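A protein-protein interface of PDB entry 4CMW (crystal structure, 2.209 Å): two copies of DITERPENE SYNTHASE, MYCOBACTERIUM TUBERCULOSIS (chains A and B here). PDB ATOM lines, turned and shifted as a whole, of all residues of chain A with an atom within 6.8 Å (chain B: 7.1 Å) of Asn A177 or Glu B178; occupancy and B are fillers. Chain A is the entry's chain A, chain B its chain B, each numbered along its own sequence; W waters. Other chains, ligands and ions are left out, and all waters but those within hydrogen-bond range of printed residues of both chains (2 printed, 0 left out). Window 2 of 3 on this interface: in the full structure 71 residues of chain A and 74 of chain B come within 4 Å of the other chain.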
ATOM      1  N   PHE A 172       7.731 -12.260   7.143  1.00  0.00           N
ATOM      2  CA  PHE A 172       7.656 -11.317   8.240  1.00  0.00           C
ATOM      3  C   PHE A 172       6.775 -10.131   7.869  1.00  0.00           C
ATOM      4  O   PHE A 172       5.963  -9.684   8.662  1.00  0.00           O
ATOM      5  CB  PHE A 172       9.049 -10.812   8.604  1.00  0.00           C
ATOM      6  CG  PHE A 172       9.029  -9.688   9.594  1.00  0.00           C
ATOM      7  CD1 PHE A 172       8.949  -9.954  10.951  1.00  0.00           C
ATOM      8  CD2 PHE A 172       9.080  -8.369   9.170  1.00  0.00           C
ATOM      9  CE1 PHE A 172       8.914  -8.922  11.876  1.00  0.00           C
ATOM     10  CE2 PHE A 172       9.052  -7.325  10.090  1.00  0.00           C
ATOM     11  CZ  PHE A 172       8.969  -7.606  11.450  1.00  0.00           C
ATOM     12  N   SER A 173       6.957  -9.610   6.665  1.00  0.00           N
ATOM     13  CA  SER A 173       6.224  -8.431   6.222  1.00  0.00           C
ATOM     14  C   SER A 173       4.742  -8.743   6.038  1.00  0.00           C
ATOM     15  O   SER A 173       3.887  -7.948   6.415  1.00  0.00           O
ATOM     16  CB  SER A 173       6.814  -7.876   4.919  1.00  0.00           C
ATOM     17  OG  SER A 173       8.180  -7.531   5.083  1.00  0.00           O
ATOM     18  N   ILE A 174       4.439  -9.905   5.468  1.00  0.00           N
ATOM     19  CA  ILE A 174       3.043 -10.331   5.365  1.00  0.00           C
ATOM     20  C   ILE A 174       2.372 -10.402   6.752  1.00  0.00           C
ATOM     21  O   ILE A 174       1.288  -9.799   6.969  1.00  0.00           O
ATOM     22  CB  ILE A 174       2.917 -11.671   4.599  1.00  0.00           C
ATOM     23  CG1 ILE A 174       3.271 -11.442   3.126  1.00  0.00           C
ATOM     24  CG2 ILE A 174       1.501 -12.287   4.748  1.00  0.00           C
ATOM     25  CD1 ILE A 174       3.660 -12.691   2.390  1.00  0.00           C
ATOM     26  N   SER A 175       3.024 -11.083   7.700  1.00  0.00           N
ATOM     27  CA  SER A 175       2.453 -11.175   9.056  1.00  0.00           C
ATOM     28  C   SER A 175       2.252  -9.790   9.658  1.00  0.00           C
ATOM     29  O   SER A 175       1.174  -9.462  10.176  1.00  0.00           O
ATOM     30  CB  SER A 175       3.345 -11.998   9.989  1.00  0.00           C
ATOM     31  OG  SER A 175       3.524 -13.308   9.488  1.00  0.00           O
ATOM     32  N   TRP A 176       3.299  -8.977   9.556  1.00  0.00           N
ATOM     33  CA  TRP A 176       3.295  -7.642  10.127  1.00  0.00           C
ATOM     34  C   TRP A 176       2.138  -6.840   9.576  1.00  0.00           C
ATOM     35  O   TRP A 176       1.424  -6.208  10.327  1.00  0.00           O
ATOM     36  CB  TRP A 176       4.603  -6.919   9.830  1.00  0.00           C
ATOM     37  CG  TRP A 176       4.714  -5.554  10.480  1.00  0.00           C
ATOM     38  CD1 TRP A 176       4.222  -4.374   9.999  1.00  0.00           C
ATOM     39  CD2 TRP A 176       5.374  -5.240  11.720  1.00  0.00           C
ATOM     40  NE1 TRP A 176       4.537  -3.343  10.859  1.00  0.00           N
ATOM     41  CE2 TRP A 176       5.247  -3.848  11.919  1.00  0.00           C
ATOM     42  CE3 TRP A 176       6.058  -5.999  12.678  1.00  0.00           C
ATOM     43  CZ2 TRP A 176       5.763  -3.202  13.050  1.00  0.00           C
ATOM     44  CZ3 TRP A 176       6.576  -5.356  13.800  1.00  0.00           C
ATOM     45  CH2 TRP A 176       6.424  -3.970  13.976  1.00  0.00           C
ATOM     46  N   ASN A 177       1.967  -6.835   8.260  1.00  0.00           N
ATOM     47  CA  ASN A 177       0.842  -6.112   7.687  1.00  0.00           C
ATOM     48  C   ASN A 177      -0.472  -6.647   8.226  1.00  0.00           C
ATOM     49  O   ASN A 177      -1.387  -5.869   8.508  1.00  0.00           O
ATOM     50  CB  ASN A 177       0.839  -6.177   6.164  1.00  0.00           C
ATOM     51  CG  ASN A 177      -0.287  -5.360   5.559  1.00  0.00           C
ATOM     52  OD1 ASN A 177      -0.230  -4.130   5.519  1.00  0.00           O
ATOM     53  ND2 ASN A 177      -1.296  -6.041   5.042  1.00  0.00           N
ATOM     54  N   GLU A 178      -0.546  -7.966   8.423  1.00  0.00           N
ATOM     55  CA  GLU A 178      -1.760  -8.548   9.004  1.00  0.00           C
ATOM     56  C   GLU A 178      -2.073  -8.008  10.403  1.00  0.00           C
ATOM     57  O   GLU A 178      -3.230  -7.731  10.704  1.00  0.00           O
ATOM     58  CB  GLU A 178      -1.699 -10.083   9.011  1.00  0.00           C
ATOM     59  CG  GLU A 178      -1.982 -10.726   7.655  1.00  0.00           C
ATOM     60  CD  GLU A 178      -1.477 -12.159   7.571  1.00  0.00           C
ATOM     61  OE1 GLU A 178      -0.884 -12.654   8.554  1.00  0.00           O
ATOM     62  OE2 GLU A 178      -1.650 -12.792   6.513  1.00  0.00           O
ATOM     63  N   THR A 179      -1.059  -7.802  11.243  1.00  0.00           N
ATOM     64  CA  THR A 179      -1.304  -7.314  12.603  1.00  0.00           C
ATOM     65  C   THR A 179      -1.375  -5.779  12.737  1.00  0.00           C
ATOM     66  O   THR A 179      -2.049  -5.258  13.613  1.00  0.00           O
ATOM     67  CB  THR A 179      -0.246  -7.865  13.577  1.00  0.00           C
ATOM     68  OG1 THR A 179      -0.082  -9.270  13.349  1.00  0.00           O
ATOM     69  CG2 THR A 179      -0.666  -7.637  15.027  1.00  0.00           C
ATOM     70  N   HIS A 180      -0.684  -5.057  11.864  1.00  0.00           N
ATOM     71  CA  HIS A 180      -0.528  -3.609  12.031  1.00  0.00           C
ATOM     72  C   HIS A 180      -1.238  -2.764  10.984  1.00  0.00           C
ATOM     73  O   HIS A 180      -1.412  -1.561  11.184  1.00  0.00           O
ATOM     74  CB  HIS A 180       0.947  -3.213  12.013  1.00  0.00           C
ATOM     75  CG  HIS A 180       1.762  -3.840  13.099  1.00  0.00           C
ATOM     76  ND1 HIS A 180       2.209  -5.141  13.038  1.00  0.00           N
ATOM     77  CD2 HIS A 180       2.220  -3.339  14.271  1.00  0.00           C
ATOM     78  CE1 HIS A 180       2.906  -5.417  14.127  1.00  0.00           C
ATOM     79  NE2 HIS A 180       2.922  -4.343  14.895  1.00  0.00           N
ATOM     80  N   GLY A 181      -1.596  -3.362   9.855  1.00  0.00           N
ATOM     81  CA  GLY A 181      -2.328  -2.631   8.839  1.00  0.00           C
ATOM     82  C   GLY A 181      -1.446  -1.831   7.911  1.00  0.00           C
ATOM     83  O   GLY A 181      -1.937  -1.133   7.023  1.00  0.00           O
ATOM     84  N   LYS A 182      -0.139  -1.910   8.122  1.00  0.00           N
ATOM     85  CA  LYS A 182       0.803  -1.258   7.226  1.00  0.00           C
ATOM     86  C   LYS A 182       2.088  -2.068   7.105  1.00  0.00           C
ATOM     87  O   LYS A 182       2.365  -2.928   7.943  1.00  0.00           O
ATOM     88  CB  LYS A 182       1.095   0.168   7.705  1.00  0.00           C
ATOM     89  CG  LYS A 182       1.638   0.260   9.111  1.00  0.00           C
ATOM     90  CD  LYS A 182       1.526   1.697   9.610  1.00  0.00           C
ATOM     91  CE  LYS A 182       2.165   1.892  10.979  1.00  0.00           C
ATOM     92  NZ  LYS A 182       2.098   3.323  11.391  1.00  0.00           N
ATOM     93  N   PRO A 183       2.868  -1.822   6.042  1.00  0.00           N
ATOM     94  CA  PRO A 183       4.121  -2.575   5.929  1.00  0.00           C
ATOM     95  C   PRO A 183       5.076  -2.214   7.069  1.00  0.00           C
ATOM     96  O   PRO A 183       4.959  -1.143   7.651  1.00  0.00           O
ATOM     97  CB  PRO A 183       4.686  -2.125   4.578  1.00  0.00           C
ATOM     98  CG  PRO A 183       3.976  -0.817   4.265  1.00  0.00           C
ATOM     99  CD  PRO A 183       2.608  -0.972   4.866  1.00  0.00           C
ATOM    100  N   PRO A 184       5.982  -3.125   7.429  1.00  0.00           N
ATOM    101  CA  PRO A 184       6.999  -2.787   8.429  1.00  0.00           C
ATOM    102  C   PRO A 184       8.027  -1.850   7.814  1.00  0.00           C
ATOM    103  O   PRO A 184       8.287  -1.970   6.616  1.00  0.00           O
ATOM    104  CB  PRO A 184       7.664  -4.126   8.711  1.00  0.00           C
ATOM    105  CG  PRO A 184       7.500  -4.901   7.413  1.00  0.00           C
ATOM    106  CD  PRO A 184       6.144  -4.485   6.890  1.00  0.00           C
ATOM    107  N   ALA B 170       9.273  -5.828   1.100  1.00  0.00           N
ATOM    108  CA  ALA B 170       8.164  -5.934   2.049  1.00  0.00           C
ATOM    109  C   ALA B 170       6.819  -5.604   1.380  1.00  0.00           C
ATOM    110  O   ALA B 170       5.830  -6.356   1.509  1.00  0.00           O
ATOM    111  CB  ALA B 170       8.410  -5.036   3.248  1.00  0.00           C
ATOM    112  N   GLN B 171       6.790  -4.491   0.648  1.00  0.00           N
ATOM    113  CA  GLN B 171       5.547  -4.060   0.004  1.00  0.00           C
ATOM    114  C   GLN B 171       5.124  -4.987  -1.154  1.00  0.00           C
ATOM    115  O   GLN B 171       3.936  -5.335  -1.297  1.00  0.00           O
ATOM    116  CB  GLN B 171       5.650  -2.602  -0.446  1.00  0.00           C
ATOM    117  CG  GLN B 171       5.893  -1.670   0.736  1.00  0.00           C
ATOM    118  CD  GLN B 171       5.890  -0.196   0.373  1.00  0.00           C
ATOM    119  OE1 GLN B 171       5.556   0.191  -0.750  1.00  0.00           O
ATOM    120  NE2 GLN B 171       6.284   0.638   1.329  1.00  0.00           N
ATOM    121  N   PHE B 172       6.107  -5.386  -1.964  1.00  0.00           N
ATOM    122  CA  PHE B 172       5.876  -6.323  -3.058  1.00  0.00           C
ATOM    123  C   PHE B 172       5.251  -7.601  -2.508  1.00  0.00           C
ATOM    124  O   PHE B 172       4.310  -8.133  -3.077  1.00  0.00           O
ATOM    125  CB  PHE B 172       7.197  -6.680  -3.754  1.00  0.00           C
ATOM    126  CG  PHE B 172       7.066  -7.801  -4.766  1.00  0.00           C
ATOM    127  CD1 PHE B 172       6.702  -7.527  -6.081  1.00  0.00           C
ATOM    128  CD2 PHE B 172       7.283  -9.136  -4.392  1.00  0.00           C
ATOM    129  CE1 PHE B 172       6.566  -8.553  -7.017  1.00  0.00           C
ATOM    130  CE2 PHE B 172       7.151 -10.169  -5.316  1.00  0.00           C
ATOM    131  CZ  PHE B 172       6.790  -9.876  -6.639  1.00  0.00           C
ATOM    132  N   SER B 173       5.805  -8.087  -1.401  1.00  0.00           N
ATOM    133  CA  SER B 173       5.378  -9.346  -0.805  1.00  0.00           C
ATOM    134  C   SER B 173       3.995  -9.248  -0.193  1.00  0.00           C
ATOM    135  O   SER B 173       3.209 -10.193  -0.315  1.00  0.00           O
ATOM    136  CB  SER B 173       6.385  -9.821   0.231  1.00  0.00           C
ATOM    137  OG  SER B 173       7.661  -9.936  -0.383  1.00  0.00           O
ATOM    138  N   ILE B 174       3.701  -8.124   0.466  1.00  0.00           N
ATOM    139  CA  ILE B 174       2.347  -7.895   0.986  1.00  0.00           C
ATOM    140  C   ILE B 174       1.307  -7.909  -0.144  1.00  0.00           C
ATOM    141  O   ILE B 174       0.260  -8.593  -0.059  1.00  0.00           O
ATOM    142  CB  ILE B 174       2.264  -6.588   1.810  1.00  0.00           C
ATOM    143  CG1 ILE B 174       3.106  -6.732   3.084  1.00  0.00           C
ATOM    144  CG2 ILE B 174       0.803  -6.209   2.133  1.00  0.00           C
ATOM    145  CD1 ILE B 174       3.520  -5.425   3.698  1.00  0.00           C
ATOM    146  N   SER B 175       1.586  -7.158  -1.206  1.00  0.00           N
ATOM    147  CA  SER B 175       0.658  -7.157  -2.341  1.00  0.00           C
ATOM    148  C   SER B 175       0.495  -8.550  -2.959  1.00  0.00           C
ATOM    149  O   SER B 175      -0.634  -9.014  -3.225  1.00  0.00           O
ATOM    150  CB  SER B 175       1.097  -6.148  -3.402  1.00  0.00           C
ATOM    151  OG  SER B 175       1.063  -4.855  -2.838  1.00  0.00           O
ATOM    152  N   TRP B 176       1.629  -9.206  -3.181  1.00  0.00           N
ATOM    153  CA  TRP B 176       1.626 -10.508  -3.804  1.00  0.00           C
ATOM    154  C   TRP B 176       0.775 -11.460  -2.997  1.00  0.00           C
ATOM    155  O   TRP B 176      -0.089 -12.119  -3.547  1.00  0.00           O
ATOM    156  CB  TRP B 176       3.028 -11.069  -3.916  1.00  0.00           C
ATOM    157  CG  TRP B 176       3.068 -12.371  -4.625  1.00  0.00           C
ATOM    158  CD1 TRP B 176       2.842 -13.613  -4.088  1.00  0.00           C
ATOM    159  CD2 TRP B 176       3.355 -12.578  -6.014  1.00  0.00           C
ATOM    160  NE1 TRP B 176       2.969 -14.578  -5.069  1.00  0.00           N
ATOM    161  CE2 TRP B 176       3.284 -13.966  -6.264  1.00  0.00           C
ATOM    162  CE3 TRP B 176       3.676 -11.723  -7.081  1.00  0.00           C
ATOM    163  CZ2 TRP B 176       3.515 -14.523  -7.524  1.00  0.00           C
ATOM    164  CZ3 TRP B 176       3.908 -12.275  -8.340  1.00  0.00           C
ATOM    165  CH2 TRP B 176       3.827 -13.662  -8.547  1.00  0.00           C
ATOM    166  N   ASN B 177       1.020 -11.527  -1.692  1.00  0.00           N
ATOM    167  CA  ASN B 177       0.241 -12.421  -0.844  1.00  0.00           C
ATOM    168  C   ASN B 177      -1.240 -12.066  -0.853  1.00  0.00           C
ATOM    169  O   ASN B 177      -2.094 -12.950  -0.748  1.00  0.00           O
ATOM    170  CB  ASN B 177       0.752 -12.420   0.582  1.00  0.00           C
ATOM    171  CG  ASN B 177       0.095 -13.485   1.428  1.00  0.00           C
ATOM    172  OD1 ASN B 177       0.440 -14.658   1.339  1.00  0.00           O
ATOM    173  ND2 ASN B 177      -0.871 -13.090   2.236  1.00  0.00           N
ATOM    174  N   GLU B 178      -1.549 -10.773  -0.936  1.00  0.00           N
ATOM    175  CA  GLU B 178      -2.953 -10.379  -1.053  1.00  0.00           C
ATOM    176  C   GLU B 178      -3.635 -10.858  -2.354  1.00  0.00           C
ATOM    177  O   GLU B 178      -4.823 -11.193  -2.351  1.00  0.00           O
ATOM    178  CB  GLU B 178      -3.128  -8.872  -0.848  1.00  0.00           C
ATOM    179  CG  GLU B 178      -3.055  -8.477   0.635  1.00  0.00           C
ATOM    180  CD  GLU B 178      -2.870  -6.988   0.856  1.00  0.00           C
ATOM    181  OE1 GLU B 178      -2.770  -6.242  -0.138  1.00  0.00           O
ATOM    182  OE2 GLU B 178      -2.837  -6.565   2.029  1.00  0.00           O
ATOM    183  N   THR B 179      -2.901 -10.885  -3.462  1.00  0.00           N
ATOM    184  CA  THR B 179      -3.508 -11.262  -4.741  1.00  0.00           C
ATOM    185  C   THR B 179      -3.315 -12.741  -5.146  1.00  0.00           C
ATOM    186  O   THR B 179      -3.937 -13.206  -6.095  1.00  0.00           O
ATOM    187  CB  THR B 179      -2.996 -10.367  -5.890  1.00  0.00           C
ATOM    188  OG1 THR B 179      -1.579 -10.529  -6.019  1.00  0.00           O
ATOM    189  CG2 THR B 179      -3.317  -8.885  -5.626  1.00  0.00           C
ATOM    190  N   HIS B 180      -2.442 -13.467  -4.455  1.00  0.00           N
ATOM    191  CA  HIS B 180      -2.156 -14.863  -4.804  1.00  0.00           C
ATOM    192  C   HIS B 180      -2.493 -15.838  -3.691  1.00  0.00           C
ATOM    193  O   HIS B 180      -2.650 -17.030  -3.926  1.00  0.00           O
ATOM    194  CB  HIS B 180      -0.690 -15.043  -5.168  1.00  0.00           C
ATOM    195  CG  HIS B 180      -0.261 -14.241  -6.351  1.00  0.00           C
ATOM    196  ND1 HIS B 180      -0.026 -12.883  -6.284  1.00  0.00           N
ATOM    197  CD2 HIS B 180      -0.005 -14.606  -7.630  1.00  0.00           C
ATOM    198  CE1 HIS B 180       0.348 -12.446  -7.474  1.00  0.00           C
ATOM    199  NE2 HIS B 180       0.371 -13.470  -8.308  1.00  0.00           N
ATOM    200  N   GLY B 181      -2.586 -15.330  -2.474  1.00  0.00           N
ATOM    201  CA  GLY B 181      -2.914 -16.165  -1.336  1.00  0.00           C
ATOM    202  C   GLY B 181      -1.767 -16.870  -0.638  1.00  0.00           C
ATOM    203  O   GLY B 181      -1.977 -17.547   0.369  1.00  0.00           O
ATOM    204  N   LYS B 182      -0.558 -16.709  -1.162  1.00  0.00           N
ATOM    205  CA  LYS B 182       0.641 -17.201  -0.487  1.00  0.00           C
ATOM    206  C   LYS B 182       1.808 -16.238  -0.763  1.00  0.00           C
ATOM    207  O   LYS B 182       1.735 -15.445  -1.696  1.00  0.00           O
ATOM    208  CB  LYS B 182       0.962 -18.637  -0.908  1.00  0.00           C
ATOM    209  CG  LYS B 182       1.154 -18.858  -2.391  1.00  0.00           C
ATOM    210  CD  LYS B 182       1.056 -20.337  -2.688  1.00  0.00           C
ATOM    211  CE  LYS B 182       1.338 -20.642  -4.139  1.00  0.00           C
ATOM    212  NZ  LYS B 182       1.263 -22.109  -4.365  1.00  0.00           N
HETATM  213  O   HOH W   1      -1.474 -15.396   4.597  1.00  0.00           O
HETATM  214  O   HOH W   2      -3.457  -4.091   4.294  1.00  0.00           O
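The side-chain amide nitrogen (ND2) of Asn A177 lies within hydrogen-bond range of the side-chain carboxylate (OE2) of Glu B178, 3.4 Å away.
Among the printed residues, pairs that only touch across the chains: Ser A173 with Ala B170 (3.1 Å), Ser A173 with Ile B174 (3.6 Å), Ile A174 with Ser B173 (3.7 Å), Ile A174 with Asn B177 (3.4 Å), Asn A177 with Ile B174 (3.6 Å) and Pro A183 with Ile B174 (3.6 Å).
Hydrophobic or aromatic side chains of chain A that line the printed part of chain B: Ile A174 and Pro A183.
Among the printed residues, 7 pairs touch across the chains.
Among the printed residues, no Asp or Glu carboxylate lies within 4 Å of a Lys or Arg side-chain nitrogen of the other chain.
The side-chain amide oxygen of Asn A177 is in hydrogen-bond range of the backbone NH of Lys A182, 3.4 Å away.
The side-chain amide oxygen (OD1) of Asn B177 lies close to the backbone NH (N) of Lys B182 (3.4 Å).
Water W2 bridges the side-chain amide nitrogen (ND2) of Asn A177 and the side-chain carboxylate (OE2) of Glu B178.
Water W1 bridges the side-chain carboxylate (OE2) of Glu A178 (3.2 Å) and the side-chain amide nitrogen (ND2) of Asn B177 (3.4 Å).
Trp A176 touches none of the printed residues of chain B.
Asn A177 touches two residues of chain B.
Printed residues of chain A within 4 Å of Ala B170: Ser A173.
Of the printed residues of chain A, Ile B174 touches Ser A173 (3.6 Å), Asn A177 (3.6 Å) and Pro A183 (3.6 Å).
Of the printed residues of chain A, Asn B177 touches Ile A174 (3.4 Å).
Printed residues of chain A within 4 Å of Glu B178: Asn A177 (3.4 Å).
The nearest residue of chain B that does not touch Asn A177 is Ala B170 (6.8 Å).
The nearest residue of chain A that does not touch Glu B178 is Ile A174 (6.3 Å).
The nearest printed residue of chain B that does not touch Ser A173 is Ser B173 (5.1 Å).
Ser A173 touches Ile B174, and with the chains exchanged Ile A174 touches Ser B173.
Ile A174 touches Asn B177, and with the chains exchanged Asn A177 touches Ile B174.
Asn A177 touches Glu B178, but with the chains exchanged Glu A178 does not touch Asn B177 (4.4 Å).
Positions printed for both chains: 172, 173, 174, 175, 176, 177, 178, 179, 180, 181 and 182.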
